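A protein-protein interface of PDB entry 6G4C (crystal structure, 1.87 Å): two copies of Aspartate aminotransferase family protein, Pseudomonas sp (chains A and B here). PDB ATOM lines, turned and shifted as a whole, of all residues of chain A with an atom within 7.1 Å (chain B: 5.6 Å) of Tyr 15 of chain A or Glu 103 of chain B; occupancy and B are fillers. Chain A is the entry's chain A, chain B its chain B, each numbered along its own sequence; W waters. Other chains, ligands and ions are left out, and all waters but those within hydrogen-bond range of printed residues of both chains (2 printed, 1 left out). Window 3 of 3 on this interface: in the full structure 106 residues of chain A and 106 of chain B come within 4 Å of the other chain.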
ATOM      1  N   PRO A   9       2.407 -12.837 -23.346  1.00  0.00           N
ATOM      2  CA  PRO A   9       2.471 -14.295 -23.291  1.00  0.00           C
ATOM      3  C   PRO A   9       3.578 -14.820 -22.382  1.00  0.00           C
ATOM      4  O   PRO A   9       3.357 -15.780 -21.654  1.00  0.00           O
ATOM      5  CB  PRO A   9       2.728 -14.709 -24.756  1.00  0.00           C
ATOM      6  CG  PRO A   9       2.252 -13.553 -25.568  1.00  0.00           C
ATOM      7  CD  PRO A   9       2.464 -12.323 -24.723  1.00  0.00           C
ATOM      8  N   GLU A  10       4.762 -14.210 -22.412  1.00  0.00           N
ATOM      9  CA  GLU A  10       5.832 -14.667 -21.527  1.00  0.00           C
ATOM     10  C   GLU A  10       5.489 -14.435 -20.059  1.00  0.00           C
ATOM     11  O   GLU A  10       5.820 -15.248 -19.225  1.00  0.00           O
ATOM     12  CB  GLU A  10       7.175 -14.060 -21.871  1.00  0.00           C
ATOM     13  CG  GLU A  10       8.302 -14.593 -21.016  1.00  0.00           C
ATOM     14  CD  GLU A  10       8.345 -16.109 -20.943  1.00  0.00           C
ATOM     15  OE1 GLU A  10       8.453 -16.763 -22.019  1.00  0.00           O
ATOM     16  OE2 GLU A  10       8.200 -16.648 -19.798  1.00  0.00           O
ATOM     17  N   LYS A  11       4.854 -13.309 -19.769  1.00  0.00           N
ATOM     18  CA  LYS A  11       4.484 -12.969 -18.405  1.00  0.00           C
ATOM     19  C   LYS A  11       3.433 -13.958 -17.918  1.00  0.00           C
ATOM     20  O   LYS A  11       3.477 -14.386 -16.776  1.00  0.00           O
ATOM     21  CB  LYS A  11       3.953 -11.523 -18.320  1.00  0.00           C
ATOM     22  CG  LYS A  11       5.023 -10.427 -18.507  1.00  0.00           C
ATOM     23  CD  LYS A  11       4.388  -9.021 -18.516  1.00  0.00           C
ATOM     24  CE  LYS A  11       5.383  -7.841 -18.789  1.00  0.00           C
ATOM     25  NZ  LYS A  11       4.891  -6.545 -18.185  1.00  0.00           N
ATOM     26  N   ASP A  12       2.501 -14.311 -18.792  1.00  0.00           N
ATOM     27  CA  ASP A  12       1.457 -15.259 -18.428  1.00  0.00           C
ATOM     28  C   ASP A  12       2.081 -16.603 -18.064  1.00  0.00           C
ATOM     29  O   ASP A  12       1.715 -17.218 -17.065  1.00  0.00           O
ATOM     30  CB  ASP A  12       0.480 -15.436 -19.581  1.00  0.00           C
ATOM     31  CG  ASP A  12      -0.605 -16.461 -19.277  1.00  0.00           C
ATOM     32  OD1 ASP A  12      -1.563 -16.138 -18.559  1.00  0.00           O
ATOM     33  OD2 ASP A  12      -0.489 -17.596 -19.740  1.00  0.00           O
ATOM     34  N   ILE A  13       3.012 -17.059 -18.908  1.00  0.00           N
ATOM     35  CA  ILE A  13       3.718 -18.309 -18.662  1.00  0.00           C
ATOM     36  C   ILE A  13       4.495 -18.270 -17.341  1.00  0.00           C
ATOM     37  O   ILE A  13       4.528 -19.256 -16.602  1.00  0.00           O
ATOM     38  CB  ILE A  13       4.697 -18.617 -19.830  1.00  0.00           C
ATOM     39  CG1 ILE A  13       3.892 -19.020 -21.085  1.00  0.00           C
ATOM     40  CG2 ILE A  13       5.683 -19.712 -19.452  1.00  0.00           C
ATOM     41  CD1 ILE A  13       4.737 -19.065 -22.344  1.00  0.00           C
ATOM     42  N   GLN A  14       5.159 -17.147 -17.076  1.00  0.00           N
ATOM     43  CA  GLN A  14       5.950 -17.002 -15.864  1.00  0.00           C
ATOM     44  C   GLN A  14       5.111 -16.992 -14.587  1.00  0.00           C
ATOM     45  O   GLN A  14       5.575 -17.509 -13.558  1.00  0.00           O
ATOM     46  CB  GLN A  14       6.784 -15.719 -15.930  1.00  0.00           C
ATOM     47  CG  GLN A  14       7.834 -15.602 -14.828  1.00  0.00           C
ATOM     48  CD  GLN A  14       8.824 -16.756 -14.846  1.00  0.00           C
ATOM     49  OE1 GLN A  14       9.373 -17.107 -15.911  1.00  0.00           O
ATOM     50  NE2 GLN A  14       9.046 -17.369 -13.680  1.00  0.00           N
ATOM     51  N   TYR A  15       3.913 -16.396 -14.635  1.00  0.00           N
ATOM     52  CA  TYR A  15       3.192 -16.059 -13.404  1.00  0.00           C
ATOM     53  C   TYR A  15       1.817 -16.686 -13.140  1.00  0.00           C
ATOM     54  O   TYR A  15       1.358 -16.670 -11.993  1.00  0.00           O
ATOM     55  CB  TYR A  15       3.030 -14.538 -13.329  1.00  0.00           C
ATOM     56  CG  TYR A  15       4.322 -13.754 -13.390  1.00  0.00           C
ATOM     57  CD1 TYR A  15       5.303 -13.910 -12.419  1.00  0.00           C
ATOM     58  CD2 TYR A  15       4.542 -12.815 -14.395  1.00  0.00           C
ATOM     59  CE1 TYR A  15       6.476 -13.157 -12.449  1.00  0.00           C
ATOM     60  CE2 TYR A  15       5.713 -12.066 -14.441  1.00  0.00           C
ATOM     61  CZ  TYR A  15       6.677 -12.239 -13.480  1.00  0.00           C
ATOM     62  OH  TYR A  15       7.844 -11.472 -13.523  1.00  0.00           O
ATOM     63  N   GLN A  16       1.145 -17.221 -14.152  1.00  0.00           N
ATOM     64  CA  GLN A  16      -0.182 -17.770 -13.925  1.00  0.00           C
ATOM     65  C   GLN A  16      -0.273 -19.270 -14.024  1.00  0.00           C
ATOM     66  O   GLN A  16       0.161 -19.867 -15.007  1.00  0.00           O
ATOM     67  CB  GLN A  16      -1.168 -17.179 -14.901  1.00  0.00           C
ATOM     68  CG  GLN A  16      -1.334 -15.703 -14.738  1.00  0.00           C
ATOM     69  CD  GLN A  16      -2.741 -15.254 -15.073  1.00  0.00           C
ATOM     70  OE1 GLN A  16      -3.615 -15.226 -14.208  1.00  0.00           O
ATOM     71  NE2 GLN A  16      -2.980 -14.969 -16.335  1.00  0.00           N
ATOM     72  N   LEU A  17      -0.858 -19.876 -13.002  1.00  0.00           N
ATOM     73  CA  LEU A  17      -1.262 -21.268 -13.058  1.00  0.00           C
ATOM     74  C   LEU A  17      -2.703 -21.313 -13.555  1.00  0.00           C
ATOM     75  O   LEU A  17      -3.620 -20.867 -12.852  1.00  0.00           O
ATOM     76  CB  LEU A  17      -1.167 -21.895 -11.673  1.00  0.00           C
ATOM     77  CG  LEU A  17      -1.684 -23.350 -11.564  1.00  0.00           C
ATOM     78  CD1 LEU A  17      -0.855 -24.294 -12.431  1.00  0.00           C
ATOM     79  CD2 LEU A  17      -1.673 -23.833 -10.126  1.00  0.00           C
ATOM     80  N   HIS A  18      -2.909 -21.835 -14.755  1.00  0.00           N
ATOM     81  CA  HIS A  18      -4.213 -21.810 -15.384  1.00  0.00           C
ATOM     82  C   HIS A  18      -5.153 -22.928 -14.946  1.00  0.00           C
ATOM     83  O   HIS A  18      -4.737 -24.065 -14.833  1.00  0.00           O
ATOM     84  CB  HIS A  18      -4.065 -21.845 -16.903  1.00  0.00           C
ATOM     85  CG  HIS A  18      -3.765 -20.501 -17.485  1.00  0.00           C
ATOM     86  ND1 HIS A  18      -4.727 -19.718 -18.081  1.00  0.00           N
ATOM     87  CD2 HIS A  18      -2.636 -19.760 -17.458  1.00  0.00           C
ATOM     88  CE1 HIS A  18      -4.188 -18.564 -18.440  1.00  0.00           C
ATOM     89  NE2 HIS A  18      -2.918 -18.568 -18.084  1.00  0.00           N
ATOM     90  N   ILE B  95      -3.014 -11.260 -16.218  1.00  0.00           N
ATOM     91  CA  ILE B  95      -1.570 -11.397 -16.401  1.00  0.00           C
ATOM     92  C   ILE B  95      -0.791 -10.339 -15.638  1.00  0.00           C
ATOM     93  O   ILE B  95       0.163 -10.662 -14.921  1.00  0.00           O
ATOM     94  CB  ILE B  95      -1.168 -11.380 -17.899  1.00  0.00           C
ATOM     95  CG1 ILE B  95      -1.766 -12.576 -18.612  1.00  0.00           C
ATOM     96  CG2 ILE B  95       0.356 -11.405 -18.044  1.00  0.00           C
ATOM     97  CD1 ILE B  95      -1.734 -12.455 -20.128  1.00  0.00           C
ATOM     98  N   ALA B  98      -1.162 -10.838 -11.879  1.00  0.00           N
ATOM     99  CA  ALA B  98      -0.355 -11.968 -11.411  1.00  0.00           C
ATOM    100  C   ALA B  98       1.133 -11.578 -11.322  1.00  0.00           C
ATOM    101  O   ALA B  98       1.807 -11.886 -10.332  1.00  0.00           O
ATOM    102  CB  ALA B  98      -0.561 -13.186 -12.303  1.00  0.00           C
ATOM    103  N   GLU B  99       1.623 -10.865 -12.329  1.00  0.00           N
ATOM    104  CA  GLU B  99       2.995 -10.309 -12.317  1.00  0.00           C
ATOM    105  C   GLU B  99       3.251  -9.467 -11.082  1.00  0.00           C
ATOM    106  O   GLU B  99       4.275  -9.642 -10.383  1.00  0.00           O
ATOM    107  CB  GLU B  99       3.244  -9.473 -13.579  1.00  0.00           C
ATOM    108  CG  GLU B  99       4.569  -8.734 -13.561  1.00  0.00           C
ATOM    109  CD  GLU B  99       4.786  -7.871 -14.802  1.00  0.00           C
ATOM    110  OE1 GLU B  99       3.864  -7.132 -15.204  1.00  0.00           O
ATOM    111  OE2 GLU B  99       5.889  -7.924 -15.358  1.00  0.00           O
ATOM    112  N   LYS B 100       2.339  -8.544 -10.815  1.00  0.00           N
ATOM    113  CA  LYS B 100       2.496  -7.616  -9.713  1.00  0.00           C
ATOM    114  C   LYS B 100       2.515  -8.352  -8.376  1.00  0.00           C
ATOM    115  O   LYS B 100       3.379  -8.079  -7.519  1.00  0.00           O
ATOM    116  CB  LYS B 100       1.408  -6.548  -9.734  1.00  0.00           C
ATOM    117  CG  LYS B 100       1.661  -5.472  -8.709  1.00  0.00           C
ATOM    118  CD  LYS B 100       0.731  -4.286  -8.891  1.00  0.00           C
ATOM    119  CE  LYS B 100       1.290  -3.090  -8.155  1.00  0.00           C
ATOM    120  NZ  LYS B 100       2.402  -2.458  -8.931  1.00  0.00           N
ATOM    121  N   LEU B 101       1.598  -9.304  -8.211  1.00  0.00           N
ATOM    122  CA  LEU B 101       1.525 -10.083  -6.972  1.00  0.00           C
ATOM    123  C   LEU B 101       2.807 -10.889  -6.734  1.00  0.00           C
ATOM    124  O   LEU B 101       3.367 -10.873  -5.629  1.00  0.00           O
ATOM    125  CB  LEU B 101       0.308 -11.018  -6.974  1.00  0.00           C
ATOM    126  CG  LEU B 101      -1.042 -10.329  -6.829  1.00  0.00           C
ATOM    127  CD1 LEU B 101      -2.165 -11.319  -7.107  1.00  0.00           C
ATOM    128  CD2 LEU B 101      -1.177  -9.731  -5.424  1.00  0.00           C
ATOM    129  N   ILE B 102       3.300 -11.560  -7.773  1.00  0.00           N
ATOM    130  CA  ILE B 102       4.526 -12.333  -7.633  1.00  0.00           C
ATOM    131  C   ILE B 102       5.705 -11.410  -7.295  1.00  0.00           C
ATOM    132  O   ILE B 102       6.506 -11.698  -6.422  1.00  0.00           O
ATOM    133  CB  ILE B 102       4.842 -13.162  -8.900  1.00  0.00           C
ATOM    134  CG1 ILE B 102       3.806 -14.280  -9.078  1.00  0.00           C
ATOM    135  CG2 ILE B 102       6.259 -13.752  -8.859  1.00  0.00           C
ATOM    136  CD1 ILE B 102       3.772 -15.308  -7.966  1.00  0.00           C
ATOM    137  N   GLU B 103       5.810 -10.291  -7.977  1.00  0.00           N
ATOM    138  CA  GLU B 103       6.978  -9.465  -7.784  1.00  0.00           C
ATOM    139  C   GLU B 103       6.929  -8.722  -6.443  1.00  0.00           C
ATOM    140  O   GLU B 103       7.976  -8.415  -5.890  1.00  0.00           O
ATOM    141  CB  GLU B 103       7.218  -8.572  -9.006  1.00  0.00           C
ATOM    142  CG  GLU B 103       7.473  -9.407 -10.283  1.00  0.00           C
ATOM    143  CD  GLU B 103       8.776 -10.225 -10.288  1.00  0.00           C
ATOM    144  OE1 GLU B 103       9.640 -10.035  -9.407  1.00  0.00           O
ATOM    145  OE2 GLU B 103       8.960 -11.057 -11.202  1.00  0.00           O
ATOM    146  N   MET B 104       5.742  -8.515  -5.871  1.00  0.00           N
ATOM    147  CA  MET B 104       5.642  -7.884  -4.553  1.00  0.00           C
ATOM    148  C   MET B 104       5.692  -8.864  -3.361  1.00  0.00           C
ATOM    149  O   MET B 104       5.758  -8.436  -2.232  1.00  0.00           O
ATOM    150  CB  MET B 104       4.389  -6.997  -4.485  1.00  0.00           C
ATOM    151  CG  MET B 104       3.068  -7.706  -4.293  1.00  0.00           C
ATOM    152  SD  MET B 104       1.714  -6.578  -4.592  1.00  0.00           S
ATOM    153  CE  MET B 104       1.781  -5.464  -3.169  1.00  0.00           C
ATOM    154  N   ALA B 105       5.680 -10.171  -3.626  1.00  0.00           N
ATOM    155  CA  ALA B 105       5.632 -11.187  -2.574  1.00  0.00           C
ATOM    156  C   ALA B 105       6.838 -11.096  -1.640  1.00  0.00           C
ATOM    157  O   ALA B 105       7.938 -10.783  -2.081  1.00  0.00           O
ATOM    158  CB  ALA B 105       5.539 -12.575  -3.169  1.00  0.00           C
ATOM    159  N   SER B 110       6.186 -18.425  -7.240  1.00  0.00           N
ATOM    160  CA  SER B 110       6.243 -18.894  -8.607  1.00  0.00           C
ATOM    161  C   SER B 110       4.999 -18.555  -9.442  1.00  0.00           C
ATOM    162  O   SER B 110       5.132 -18.036 -10.570  1.00  0.00           O
ATOM    163  CB  SER B 110       6.518 -20.397  -8.611  1.00  0.00           C
ATOM    164  OG  SER B 110       6.499 -20.943  -9.925  1.00  0.00           O
ATOM    165  N   LYS B 111       3.808 -18.858  -8.916  1.00  0.00           N
ATOM    166  CA  LYS B 111       2.566 -18.727  -9.684  1.00  0.00           C
ATOM    167  C   LYS B 111       1.421 -18.213  -8.844  1.00  0.00           C
ATOM    168  O   LYS B 111       1.414 -18.351  -7.623  1.00  0.00           O
ATOM    169  CB  LYS B 111       2.146 -20.087 -10.250  1.00  0.00           C
ATOM    170  CG  LYS B 111       3.156 -20.747 -11.187  1.00  0.00           C
ATOM    171  CD  LYS B 111       3.300 -20.010 -12.521  1.00  0.00           C
ATOM    172  CE  LYS B 111       4.481 -20.548 -13.345  1.00  0.00           C
ATOM    173  NZ  LYS B 111       5.797 -20.104 -12.792  1.00  0.00           N
ATOM    174  N   VAL B 112       0.444 -17.624  -9.522  1.00  0.00           N
ATOM    175  CA  VAL B 112      -0.799 -17.179  -8.928  1.00  0.00           C
ATOM    176  C   VAL B 112      -1.943 -17.987  -9.504  1.00  0.00           C
ATOM    177  O   VAL B 112      -2.001 -18.221 -10.715  1.00  0.00           O
ATOM    178  CB  VAL B 112      -1.051 -15.691  -9.268  1.00  0.00           C
ATOM    179  CG1 VAL B 112      -2.328 -15.202  -8.620  1.00  0.00           C
ATOM    180  CG2 VAL B 112       0.121 -14.834  -8.814  1.00  0.00           C
HETATM  181  O   HOH W   1       8.091  -9.397 -15.133  1.00  0.00           O
HETATM  182  O   HOH W   2       7.596 -16.934 -11.223  1.00  0.00           O
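The backbone NH of Leu 17 of chain A lies within hydrogen-bond range of the backbone carbonyl oxygen of Val 112 of chain B (3.0 Å). OE1 of Glu 99 of chain B lies within salt-bridge range of NZ of Lys 11 of chain A, at 3.2 Å. O of Ser 110 of chain B lies close to O of Gln 14 of chain A, 3.1 Å away. The backbone carbonyl oxygen (O) of Tyr 15 of chain A lies within hydrogen-bond range of the backbone NH (N) of Val 112 of chain B, 2.8 Å away. The side-chain amino group (NZ) of Lys 111 of chain B is in hydrogen-bond range of the backbone carbonyl oxygen (O) of Gln 14 of chain A, 2.7 Å away. OH of Tyr 15 of chain A lies within hydrogen-bond range of OE2 of Glu 103 of chain B.
A ring nitrogen (NE2) of His 18 of chain A sits at hydrogen-bond distance from the side-chain carboxylate of Asp 12 of chain A (2.8 Å). The side-chain hydroxyl (OG) of Ser 110 of chain B is in hydrogen-bond range of the side-chain amino group (NZ) of Lys 111 of chain B (3.1 Å). OD1 of Asp 12 of chain A is in hydrogen-bond range of NE2 of Gln 16 of chain A.
Among the printed residues, pairs that only touch across the chains: Tyr 15 of chain A with Lys 111 of chain B, Ile 13 of chain A with Lys 111 of chain B, Gln 16 of chain A with Ile 95 of chain B, Asp 12 of chain A with Ile 95 of chain B, Gln 16 of chain A with Ala 98 of chain B, Tyr 15 of chain A with Glu 99 of chain B, Lys 11 of chain A with Ile 95 of chain B, Tyr 15 of chain A with Ile 102 of chain B, Gln 16 of chain A with Val 112 of chain B, Gln 16 of chain A with Lys 111 of chain B, Tyr 15 of chain A with Ser 110 of chain B and Tyr 15 of chain A with Ala 98 of chain B.
Tyr 15 of chain A touches just these residues of chain B: Ala 98, Glu 99, Ile 102, Glu 103, Ser 110, Lys 111 and Val 112. Of chain A, only Tyr 15 (2.6 Å) comes within 4 Å of Glu 103 of chain B. Printed residues of chain A within 4 Å of Ala 98 of chain B: Tyr 15 and Gln 16. Printed residues of chain B within 4 Å of Lys 11 of chain A: Ile 95 (3.6 Å) and Glu 99 (3.2 Å). Of the printed residues of chain B, Ile 13 of chain A touches Lys 111 (3.5 Å). Of the printed residues of chain B, Asp 12 of chain A touches Ile 95. Glu 10 of chain A touches none of the printed residues of chain B. Leu 101 of chain B touches none of the printed residues of chain A. The nearest residue of chain A that does not touch Glu 103 of chain B is Gln 14 of chain A (5.9 Å).
Of the 12 printed residues of chain B, 8 touch a printed residue of chain A. Printed residues of chain B that touch a printed residue of chain A: Ile 95, Ala 98, Glu 99, Ile 102, Glu 103, Ser 110, Lys 111 and Val 112. Of the 10 printed residues of chain A, 7 touch a printed residue of chain B. Printed residues of chain A that touch a printed residue of chain B: Lys 11, Asp 12, Ile 13, Gln 14, Tyr 15, Gln 16 and Leu 17. Hydrophobic or aromatic side chains of chain A within 4 Å of the printed part of chain B: Tyr 15 and Leu 17. Among the printed residues, 18 pairs touch across the chains. Among the printed residues, Asp or Glu carboxylates within 4 Å of a Lys or Arg side-chain nitrogen of the other chain: Lys 11 of chain A with Glu 99 of chain B.
No position is printed for both chains. Of the 18 pairs that touch across the chains among the printed residues, none has its exchanged pair printed and touching as well.
Water W1 bridges the side-chain hydroxyl (OH) of Tyr 15 of chain A and the side-chain carboxylate (OE2) of Glu 99 of chain B. Water W2 lies within hydrogen-bond range of O of Ser 110 of chain B (2.8 Å) and NE2 of Gln 14 of chain A (2.9 Å).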
